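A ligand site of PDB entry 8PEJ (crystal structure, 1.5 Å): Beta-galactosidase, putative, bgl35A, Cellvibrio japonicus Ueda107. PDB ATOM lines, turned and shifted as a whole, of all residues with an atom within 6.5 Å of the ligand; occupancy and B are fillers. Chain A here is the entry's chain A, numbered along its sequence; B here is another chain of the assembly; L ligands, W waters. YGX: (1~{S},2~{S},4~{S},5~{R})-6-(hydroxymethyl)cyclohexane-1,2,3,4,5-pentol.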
ATOM      1  N   GLN A  39       7.512 -28.218   0.405  1.00  0.00           N
ATOM      2  CA  GLN A  39       6.880 -28.676  -0.832  1.00  0.00           C
ATOM      3  C   GLN A  39       7.624 -29.887  -1.343  1.00  0.00           C
ATOM      4  O   GLN A  39       8.873 -29.910  -1.380  1.00  0.00           O
ATOM      5  CB  GLN A  39       6.769 -27.581  -1.899  1.00  0.00           C
ATOM      6  CG  GLN A  39       6.144 -28.053  -3.161  1.00  0.00           C
ATOM      7  CD  GLN A  39       5.786 -27.047  -4.259  1.00  0.00           C
ATOM      8  OE1 GLN A  39       5.602 -27.487  -5.378  1.00  0.00           O
ATOM      9  NE2 GLN A  39       5.757 -25.775  -3.911  1.00  0.00           N
ATOM     10  N   THR A  40       6.894 -30.918  -1.743  1.00  0.00           N
ATOM     11  CA  THR A  40       7.501 -32.128  -2.265  1.00  0.00           C
ATOM     12  C   THR A  40       8.069 -31.897  -3.675  1.00  0.00           C
ATOM     13  O   THR A  40       7.716 -30.972  -4.360  1.00  0.00           O
ATOM     14  CB  THR A  40       6.464 -33.262  -2.345  1.00  0.00           C
ATOM     15  OG1 THR A  40       5.455 -33.005  -3.326  1.00  0.00           O
ATOM     16  CG2 THR A  40       5.793 -33.541  -1.016  1.00  0.00           C
ATOM     17  N   ASN A  41       8.918 -32.833  -4.102  1.00  0.00           N
ATOM     18  CA  ASN A  41       9.195 -33.020  -5.517  1.00  0.00           C
ATOM     19  C   ASN A  41       7.911 -33.411  -6.242  1.00  0.00           C
ATOM     20  O   ASN A  41       6.895 -33.799  -5.634  1.00  0.00           O
ATOM     21  CB  ASN A  41      10.364 -33.984  -5.690  1.00  0.00           C
ATOM     22  CG  ASN A  41      11.714 -33.357  -5.447  1.00  0.00           C
ATOM     23  OD1 ASN A  41      12.082 -32.418  -6.169  1.00  0.00           O
ATOM     24  ND2 ASN A  41      12.442 -33.828  -4.445  1.00  0.00           N
ATOM     25  N   ASN A  42       7.978 -33.355  -7.566  1.00  0.00           N
ATOM     26  CA  ASN A  42       6.819 -33.470  -8.447  1.00  0.00           C
ATOM     27  C   ASN A  42       6.238 -34.873  -8.582  1.00  0.00           C
ATOM     28  O   ASN A  42       5.118 -34.991  -9.115  1.00  0.00           O
ATOM     29  CB  ASN A  42       7.208 -32.996  -9.844  1.00  0.00           C
ATOM     30  CG  ASN A  42       7.321 -31.504 -10.057  1.00  0.00           C
ATOM     31  OD1 ASN A  42       7.792 -31.109 -11.137  1.00  0.00           O
ATOM     32  ND2 ASN A  42       6.904 -30.652  -9.129  1.00  0.00           N
ATOM     33  N   LEU A 103      -1.890 -28.828  -4.526  1.00  0.00           N
ATOM     34  CA  LEU A 103      -1.516 -28.213  -5.805  1.00  0.00           C
ATOM     35  C   LEU A 103      -2.237 -28.968  -6.901  1.00  0.00           C
ATOM     36  O   LEU A 103      -1.897 -30.088  -7.225  1.00  0.00           O
ATOM     37  CB  LEU A 103       0.000 -28.246  -5.990  1.00  0.00           C
ATOM     38  CG  LEU A 103       0.872 -27.869  -4.784  1.00  0.00           C
ATOM     39  CD1 LEU A 103       2.339 -28.033  -5.133  1.00  0.00           C
ATOM     40  CD2 LEU A 103       0.590 -26.482  -4.251  1.00  0.00           C
ATOM     41  N   PHE A 105      -2.699 -29.996 -10.290  1.00  0.00           N
ATOM     42  CA  PHE A 105      -1.906 -30.130 -11.506  1.00  0.00           C
ATOM     43  C   PHE A 105      -2.842 -30.656 -12.589  1.00  0.00           C
ATOM     44  O   PHE A 105      -3.259 -31.789 -12.519  1.00  0.00           O
ATOM     45  CB  PHE A 105      -0.740 -31.108 -11.315  1.00  0.00           C
ATOM     46  CG  PHE A 105       0.473 -30.625 -10.558  1.00  0.00           C
ATOM     47  CD1 PHE A 105       0.500 -29.462  -9.786  1.00  0.00           C
ATOM     48  CD2 PHE A 105       1.628 -31.420 -10.560  1.00  0.00           C
ATOM     49  CE1 PHE A 105       1.662 -29.071  -9.131  1.00  0.00           C
ATOM     50  CE2 PHE A 105       2.797 -31.023  -9.911  1.00  0.00           C
ATOM     51  CZ  PHE A 105       2.804 -29.864  -9.187  1.00  0.00           C
ATOM     52  N   LYS A 109       0.755 -27.481 -15.955  1.00  0.00           N
ATOM     53  CA  LYS A 109       1.830 -27.662 -14.984  1.00  0.00           C
ATOM     54  C   LYS A 109       3.084 -27.273 -15.725  1.00  0.00           C
ATOM     55  O   LYS A 109       3.520 -27.968 -16.668  1.00  0.00           O
ATOM     56  CB  LYS A 109       1.852 -29.108 -14.445  1.00  0.00           C
ATOM     57  CG  LYS A 109       2.779 -29.371 -13.245  1.00  0.00           C
ATOM     58  CD  LYS A 109       4.233 -29.107 -13.502  1.00  0.00           C
ATOM     59  CE  LYS A 109       5.103 -29.487 -12.309  1.00  0.00           C
ATOM     60  NZ  LYS A 109       6.528 -29.095 -12.557  1.00  0.00           N
ATOM     61  N   ASN A 110       3.673 -26.124 -15.365  1.00  0.00           N
ATOM     62  CA  ASN A 110       4.850 -25.570 -16.017  1.00  0.00           C
ATOM     63  C   ASN A 110       4.557 -25.480 -17.524  1.00  0.00           C
ATOM     64  O   ASN A 110       5.336 -25.987 -18.328  1.00  0.00           O
ATOM     65  CB  ASN A 110       6.131 -26.379 -15.733  1.00  0.00           C
ATOM     66  CG  ASN A 110       6.652 -26.260 -14.296  1.00  0.00           C
ATOM     67  OD1 ASN A 110       5.883 -26.114 -13.361  1.00  0.00           O
ATOM     68  ND2 ASN A 110       7.963 -26.293 -14.117  1.00  0.00           N
ATOM     69  N   GLN A 176      -3.916 -24.544  -4.622  1.00  0.00           N
ATOM     70  CA  GLN A 176      -3.310 -23.857  -5.774  1.00  0.00           C
ATOM     71  C   GLN A 176      -3.980 -24.374  -7.044  1.00  0.00           C
ATOM     72  O   GLN A 176      -4.039 -25.590  -7.244  1.00  0.00           O
ATOM     73  CB  GLN A 176      -1.823 -24.192  -5.829  1.00  0.00           C
ATOM     74  CG  GLN A 176      -1.061 -23.331  -6.832  1.00  0.00           C
ATOM     75  CD  GLN A 176       0.351 -23.844  -6.906  1.00  0.00           C
ATOM     76  OE1 GLN A 176       1.247 -23.477  -6.119  1.00  0.00           O
ATOM     77  NE2 GLN A 176       0.547 -24.761  -7.826  1.00  0.00           N
ATOM     78  N   ASN A 179      -0.478 -25.157 -11.976  1.00  0.00           N
ATOM     79  CA  ASN A 179       0.856 -24.892 -11.501  1.00  0.00           C
ATOM     80  C   ASN A 179       1.654 -24.202 -12.591  1.00  0.00           C
ATOM     81  O   ASN A 179       1.900 -24.796 -13.670  1.00  0.00           O
ATOM     82  CB  ASN A 179       1.560 -26.197 -11.079  1.00  0.00           C
ATOM     83  CG  ASN A 179       2.888 -25.956 -10.391  1.00  0.00           C
ATOM     84  OD1 ASN A 179       2.942 -25.783  -9.186  1.00  0.00           O
ATOM     85  ND2 ASN A 179       3.973 -25.954 -11.148  1.00  0.00           N
ATOM     86  N   GLU A 180       2.071 -22.963 -12.375  1.00  0.00           N
ATOM     87  CA  GLU A 180       2.838 -22.215 -13.364  1.00  0.00           C
ATOM     88  C   GLU A 180       2.187 -22.262 -14.763  1.00  0.00           C
ATOM     89  O   GLU A 180       2.747 -22.825 -15.718  1.00  0.00           O
ATOM     90  CB  GLU A 180       4.328 -22.617 -13.393  1.00  0.00           C
ATOM     91  CG  GLU A 180       5.048 -22.280 -12.108  1.00  0.00           C
ATOM     92  CD  GLU A 180       6.556 -22.277 -12.130  1.00  0.00           C
ATOM     93  OE1 GLU A 180       7.140 -22.820 -13.092  1.00  0.00           O
ATOM     94  OE2 GLU A 180       7.193 -21.688 -11.144  1.00  0.00           O
ATOM     95  N   ASN A 256       0.352 -19.676  -8.819  1.00  0.00           N
ATOM     96  CA  ASN A 256       1.793 -19.497  -8.652  1.00  0.00           C
ATOM     97  C   ASN A 256       2.483 -19.191  -9.986  1.00  0.00           C
ATOM     98  O   ASN A 256       2.346 -19.895 -10.996  1.00  0.00           O
ATOM     99  CB  ASN A 256       2.425 -20.728  -7.988  1.00  0.00           C
ATOM    100  CG  ASN A 256       2.401 -21.957  -8.864  1.00  0.00           C
ATOM    101  OD1 ASN A 256       1.415 -22.211  -9.541  1.00  0.00           O
ATOM    102  ND2 ASN A 256       3.432 -22.760  -8.777  1.00  0.00           N
ATOM    103  N   ASP A 297       7.085 -17.629  -7.541  1.00  0.00           N
ATOM    104  CA  ASP A 297       7.953 -18.780  -7.400  1.00  0.00           C
ATOM    105  C   ASP A 297       9.382 -18.305  -7.610  1.00  0.00           C
ATOM    106  O   ASP A 297       9.694 -17.871  -8.723  1.00  0.00           O
ATOM    107  CB  ASP A 297       7.597 -19.830  -8.441  1.00  0.00           C
ATOM    108  CG  ASP A 297       6.278 -20.536  -8.180  1.00  0.00           C
ATOM    109  OD1 ASP A 297       5.656 -20.295  -7.119  1.00  0.00           O
ATOM    110  OD2 ASP A 297       5.856 -21.332  -9.041  1.00  0.00           O
ATOM    111  N   TYR A 299      13.421 -18.652  -7.829  1.00  0.00           N
ATOM    112  CA  TYR A 299      14.672 -19.404  -7.937  1.00  0.00           C
ATOM    113  C   TYR A 299      15.858 -18.493  -8.264  1.00  0.00           C
ATOM    114  O   TYR A 299      17.005 -18.946  -8.360  1.00  0.00           O
ATOM    115  CB  TYR A 299      14.531 -20.558  -8.928  1.00  0.00           C
ATOM    116  CG  TYR A 299      14.258 -21.895  -8.261  1.00  0.00           C
ATOM    117  CD1 TYR A 299      15.254 -22.561  -7.553  1.00  0.00           C
ATOM    118  CD2 TYR A 299      13.012 -22.496  -8.370  1.00  0.00           C
ATOM    119  CE1 TYR A 299      15.020 -23.772  -6.929  1.00  0.00           C
ATOM    120  CE2 TYR A 299      12.753 -23.693  -7.723  1.00  0.00           C
ATOM    121  CZ  TYR A 299      13.756 -24.340  -7.023  1.00  0.00           C
ATOM    122  OH  TYR A 299      13.570 -25.563  -6.413  1.00  0.00           O
ATOM    123  N   GLU A 324       6.950 -21.117  -3.883  1.00  0.00           N
ATOM    124  CA  GLU A 324       8.042 -22.011  -4.242  1.00  0.00           C
ATOM    125  C   GLU A 324       9.301 -21.183  -4.078  1.00  0.00           C
ATOM    126  O   GLU A 324       9.333 -20.034  -4.516  1.00  0.00           O
ATOM    127  CB  GLU A 324       7.882 -22.463  -5.708  1.00  0.00           C
ATOM    128  CG  GLU A 324       9.005 -23.365  -6.227  1.00  0.00           C
ATOM    129  CD  GLU A 324       9.066 -23.301  -7.741  1.00  0.00           C
ATOM    130  OE1 GLU A 324       8.726 -24.475  -8.307  1.00  0.00           O
ATOM    131  OE2 GLU A 324       9.697 -22.351  -8.422  1.00  0.00           O
ATOM    132  N   PHE A 349      11.091 -25.773  -2.049  1.00  0.00           N
ATOM    133  CA  PHE A 349      10.746 -26.831  -2.952  1.00  0.00           C
ATOM    134  C   PHE A 349      11.745 -27.976  -2.857  1.00  0.00           C
ATOM    135  O   PHE A 349      12.949 -27.783  -2.693  1.00  0.00           O
ATOM    136  CB  PHE A 349      10.766 -26.273  -4.373  1.00  0.00           C
ATOM    137  CG  PHE A 349      10.375 -27.286  -5.414  1.00  0.00           C
ATOM    138  CD1 PHE A 349       9.044 -27.560  -5.648  1.00  0.00           C
ATOM    139  CD2 PHE A 349      11.315 -28.094  -6.013  1.00  0.00           C
ATOM    140  CE1 PHE A 349       8.669 -28.541  -6.540  1.00  0.00           C
ATOM    141  CE2 PHE A 349      10.929 -29.069  -6.912  1.00  0.00           C
ATOM    142  CZ  PHE A 349       9.604 -29.310  -7.158  1.00  0.00           C
ATOM    143  N   TYR A 356      15.859 -37.188  -6.036  1.00  0.00           N
ATOM    144  CA  TYR A 356      15.846 -36.231  -7.117  1.00  0.00           C
ATOM    145  C   TYR A 356      16.352 -34.889  -6.587  1.00  0.00           C
ATOM    146  O   TYR A 356      16.003 -34.493  -5.467  1.00  0.00           O
ATOM    147  CB  TYR A 356      14.468 -36.033  -7.728  1.00  0.00           C
ATOM    148  CG  TYR A 356      14.511 -35.104  -8.907  1.00  0.00           C
ATOM    149  CD1 TYR A 356      14.746 -35.563 -10.193  1.00  0.00           C
ATOM    150  CD2 TYR A 356      14.242 -33.747  -8.734  1.00  0.00           C
ATOM    151  CE1 TYR A 356      14.827 -34.736 -11.286  1.00  0.00           C
ATOM    152  CE2 TYR A 356      14.255 -32.930  -9.843  1.00  0.00           C
ATOM    153  CZ  TYR A 356      14.574 -33.397 -11.095  1.00  0.00           C
ATOM    154  OH  TYR A 356      14.645 -32.575 -12.205  1.00  0.00           O
ATOM    155  N   ASN A 358      16.885 -30.845  -8.362  1.00  0.00           N
ATOM    156  CA  ASN A 358      16.803 -29.964  -9.513  1.00  0.00           C
ATOM    157  C   ASN A 358      18.015 -29.032  -9.598  1.00  0.00           C
ATOM    158  O   ASN A 358      17.950 -28.020 -10.337  1.00  0.00           O
ATOM    159  CB  ASN A 358      15.498 -29.153  -9.519  1.00  0.00           C
ATOM    160  CG  ASN A 358      15.385 -28.201  -8.347  1.00  0.00           C
ATOM    161  OD1 ASN A 358      16.297 -28.051  -7.551  1.00  0.00           O
ATOM    162  ND2 ASN A 358      14.234 -27.572  -8.197  1.00  0.00           N
ATOM    163  N   LEU A 361      19.137 -25.470  -9.900  1.00  0.00           N
ATOM    164  CA  LEU A 361      18.156 -24.596  -9.280  1.00  0.00           C
ATOM    165  C   LEU A 361      18.303 -24.685  -7.756  1.00  0.00           C
ATOM    166  O   LEU A 361      18.531 -23.698  -7.051  1.00  0.00           O
ATOM    167  CB  LEU A 361      16.751 -25.003  -9.748  1.00  0.00           C
ATOM    168  CG  LEU A 361      16.383 -24.619 -11.176  1.00  0.00           C
ATOM    169  CD1 LEU A 361      14.911 -24.873 -11.461  1.00  0.00           C
ATOM    170  CD2 LEU A 361      16.685 -23.154 -11.497  1.00  0.00           C
ATOM    171  N   PHE B 454      18.333 -32.057 -14.161  1.00  0.00           N
ATOM    172  CA  PHE B 454      17.499 -30.951 -14.576  1.00  0.00           C
ATOM    173  C   PHE B 454      18.233 -30.136 -15.645  1.00  0.00           C
ATOM    174  O   PHE B 454      19.450 -30.028 -15.575  1.00  0.00           O
ATOM    175  CB  PHE B 454      17.183 -30.086 -13.342  1.00  0.00           C
ATOM    176  CG  PHE B 454      16.141 -29.024 -13.558  1.00  0.00           C
ATOM    177  CD1 PHE B 454      16.475 -27.811 -14.136  1.00  0.00           C
ATOM    178  CD2 PHE B 454      14.832 -29.243 -13.173  1.00  0.00           C
ATOM    179  CE1 PHE B 454      15.495 -26.833 -14.333  1.00  0.00           C
ATOM    180  CE2 PHE B 454      13.851 -28.269 -13.356  1.00  0.00           C
ATOM    181  CZ  PHE B 454      14.186 -27.076 -13.954  1.00  0.00           C
ATOM    182  N   GLY B 524       6.320 -34.423 -14.443  1.00  0.00           N
ATOM    183  CA  GLY B 524       6.859 -33.108 -14.093  1.00  0.00           C
ATOM    184  C   GLY B 524       8.365 -33.098 -14.282  1.00  0.00           C
ATOM    185  O   GLY B 524       8.908 -33.633 -15.246  1.00  0.00           O
ATOM    186  N   ASP B 525       9.071 -32.561 -13.290  1.00  0.00           N
ATOM    187  CA  ASP B 525      10.498 -32.480 -13.305  1.00  0.00           C
ATOM    188  C   ASP B 525      11.146 -33.837 -13.577  1.00  0.00           C
ATOM    189  O   ASP B 525      12.234 -33.878 -14.111  1.00  0.00           O
ATOM    190  CB  ASP B 525      11.075 -31.985 -11.961  1.00  0.00           C
ATOM    191  CG  ASP B 525      10.726 -30.564 -11.528  1.00  0.00           C
ATOM    192  OD1 ASP B 525      10.358 -29.728 -12.386  1.00  0.00           O
ATOM    193  OD2 ASP B 525      10.820 -30.324 -10.316  1.00  0.00           O
ATOM    194  N   ASP B 528      10.620 -34.281 -17.468  1.00  0.00           N
ATOM    195  CA  ASP B 528      10.901 -33.164 -18.385  1.00  0.00           C
ATOM    196  C   ASP B 528      12.275 -33.191 -19.059  1.00  0.00           C
ATOM    197  O   ASP B 528      12.442 -32.664 -20.166  1.00  0.00           O
ATOM    198  CB  ASP B 528      10.838 -31.849 -17.633  1.00  0.00           C
ATOM    199  CG  ASP B 528       9.471 -31.282 -17.408  1.00  0.00           C
ATOM    200  OD1 ASP B 528       8.479 -31.666 -18.157  1.00  0.00           O
ATOM    201  OD2 ASP B 528       9.412 -30.458 -16.464  1.00  0.00           O
HETATM  202  O4' YGX L   1       9.875 -24.902 -11.798  1.00  0.00           O
HETATM  203  O7  YGX L   1       8.933 -27.616 -11.589  1.00  0.00           O
HETATM  204  C1' YGX L   1       7.822 -26.852  -9.606  1.00  0.00           C
HETATM  205  C2' YGX L   1       7.504 -25.453 -10.132  1.00  0.00           C
HETATM  206  O2' YGX L   1       6.228 -25.017  -9.619  1.00  0.00           O
HETATM  207  C3' YGX L   1       8.631 -24.525  -9.769  1.00  0.00           C
HETATM  208  C4' YGX L   1       9.967 -24.973 -10.375  1.00  0.00           C
HETATM  209  C5' YGX L   1      10.279 -26.413  -9.979  1.00  0.00           C
HETATM  210  O6' YGX L   1      12.145 -28.011 -10.011  1.00  0.00           O
HETATM  211  C6' YGX L   1      11.606 -26.861 -10.616  1.00  0.00           C
HETATM  212  C7' YGX L   1       9.115 -27.378 -10.179  1.00  0.00           C
HETATM  213  O1' YGX L   1       6.743 -27.784  -9.782  1.00  0.00           O
HETATM  214  O   HOH W   1       9.656 -22.373 -13.348  1.00  0.00           O
HETATM  215  O   HOH W   2       4.851 -27.465  -7.907  1.00  0.00           O
HETATM  216  O   HOH W   3       5.889 -24.630  -6.935  1.00  0.00           O
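A carbon (C3') of the ligand is bonded to the side-chain carboxylate (OE1) of Glu 324 (1.5 Å).
An oxygen (O7) of the ligand sits at hydrogen-bond distance from the side-chain carboxylate (OD1) of Asp 525 of chain B (2.7 Å).
The side-chain amide nitrogen (ND2) of Asn 358 sits at hydrogen-bond distance from an oxygen (O6') of the ligand.
ND2 of Asn 179 lies within hydrogen-bond range of O2' of the ligand, at 2.9 Å.
ND2 of Asn 42 lies within hydrogen-bond range of O1' of the ligand, at 2.9 Å.
The side-chain amino group (NZ) of Lys 109 sits at hydrogen-bond distance from an oxygen (O7) of the ligand, 3.0 Å away.
An oxygen (O7) of the ligand lies within hydrogen-bond range of the side-chain amide nitrogen (ND2) of Asn 110.
N of Asp 525 of chain B sits at hydrogen-bond distance from OD1 of Asn 42, at 2.9 Å.
O of Asn 179 sits at hydrogen-bond distance from N of Asn 110.
The side-chain amide oxygen (OD1) of Asn 179 lies within hydrogen-bond range of the side-chain amide nitrogen (ND2) of Asn 256, 3.1 Å away.
The side-chain amide oxygen (OD1) of Asn 42 is in hydrogen-bond range of the side-chain amino group (NZ) of Lys 109, at 2.8 Å.
OD1 of Asn 110 sits at hydrogen-bond distance from NZ of Lys 109 (3.2 Å).
The backbone NH (N) of Glu 180 lies within hydrogen-bond range of the side-chain amide oxygen (OD1) of Asn 256.
The side-chain carboxylate (OD2) of Asp 297 is in hydrogen-bond range of the side-chain amide nitrogen (ND2) of Asn 256.
NE2 of Gln 176 lies within hydrogen-bond range of OD1 of Asn 256 (3.2 Å).
Glu 180 touches the ligand (OE2 to C3', 3.5 Å).
Asn 256 touches the ligand.
Asp 297 touches the ligand.
CE2 of Phe 349 touches O6' of the ligand, at 3.5 Å.
Leu 361 touches the ligand (CD1 to C6', 3.9 Å).
Phe 454 of chain B touches the ligand.
13 residues have an atom within 4 Å of the ligand: Asn 42, Lys 109, Asn 110, Asn 179, Glu 180, Asn 256, Asp 297, Glu 324, Phe 349, Asn 358, Leu 361, Phe 454 of chain B and Asp 525 of chain B.
Water W2 lies within hydrogen-bond range of the side-chain amide oxygen (OE1) of Gln 39, an oxygen (O1') of the ligand and the side-chain amide oxygen (OD1) of Asn 179.
Water W3 lies within hydrogen-bond range of an oxygen (O2') of the ligand (2.7 Å), the side-chain carboxylate (OE1) of Glu 324 (3.2 Å) and the side-chain amide nitrogen (NE2) of Gln 39 (3.2 Å).
Water W1 lies within hydrogen-bond range of the side-chain carboxylate of Glu 180 (2.6 Å) and an oxygen (O4') of the ligand (3.0 Å).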
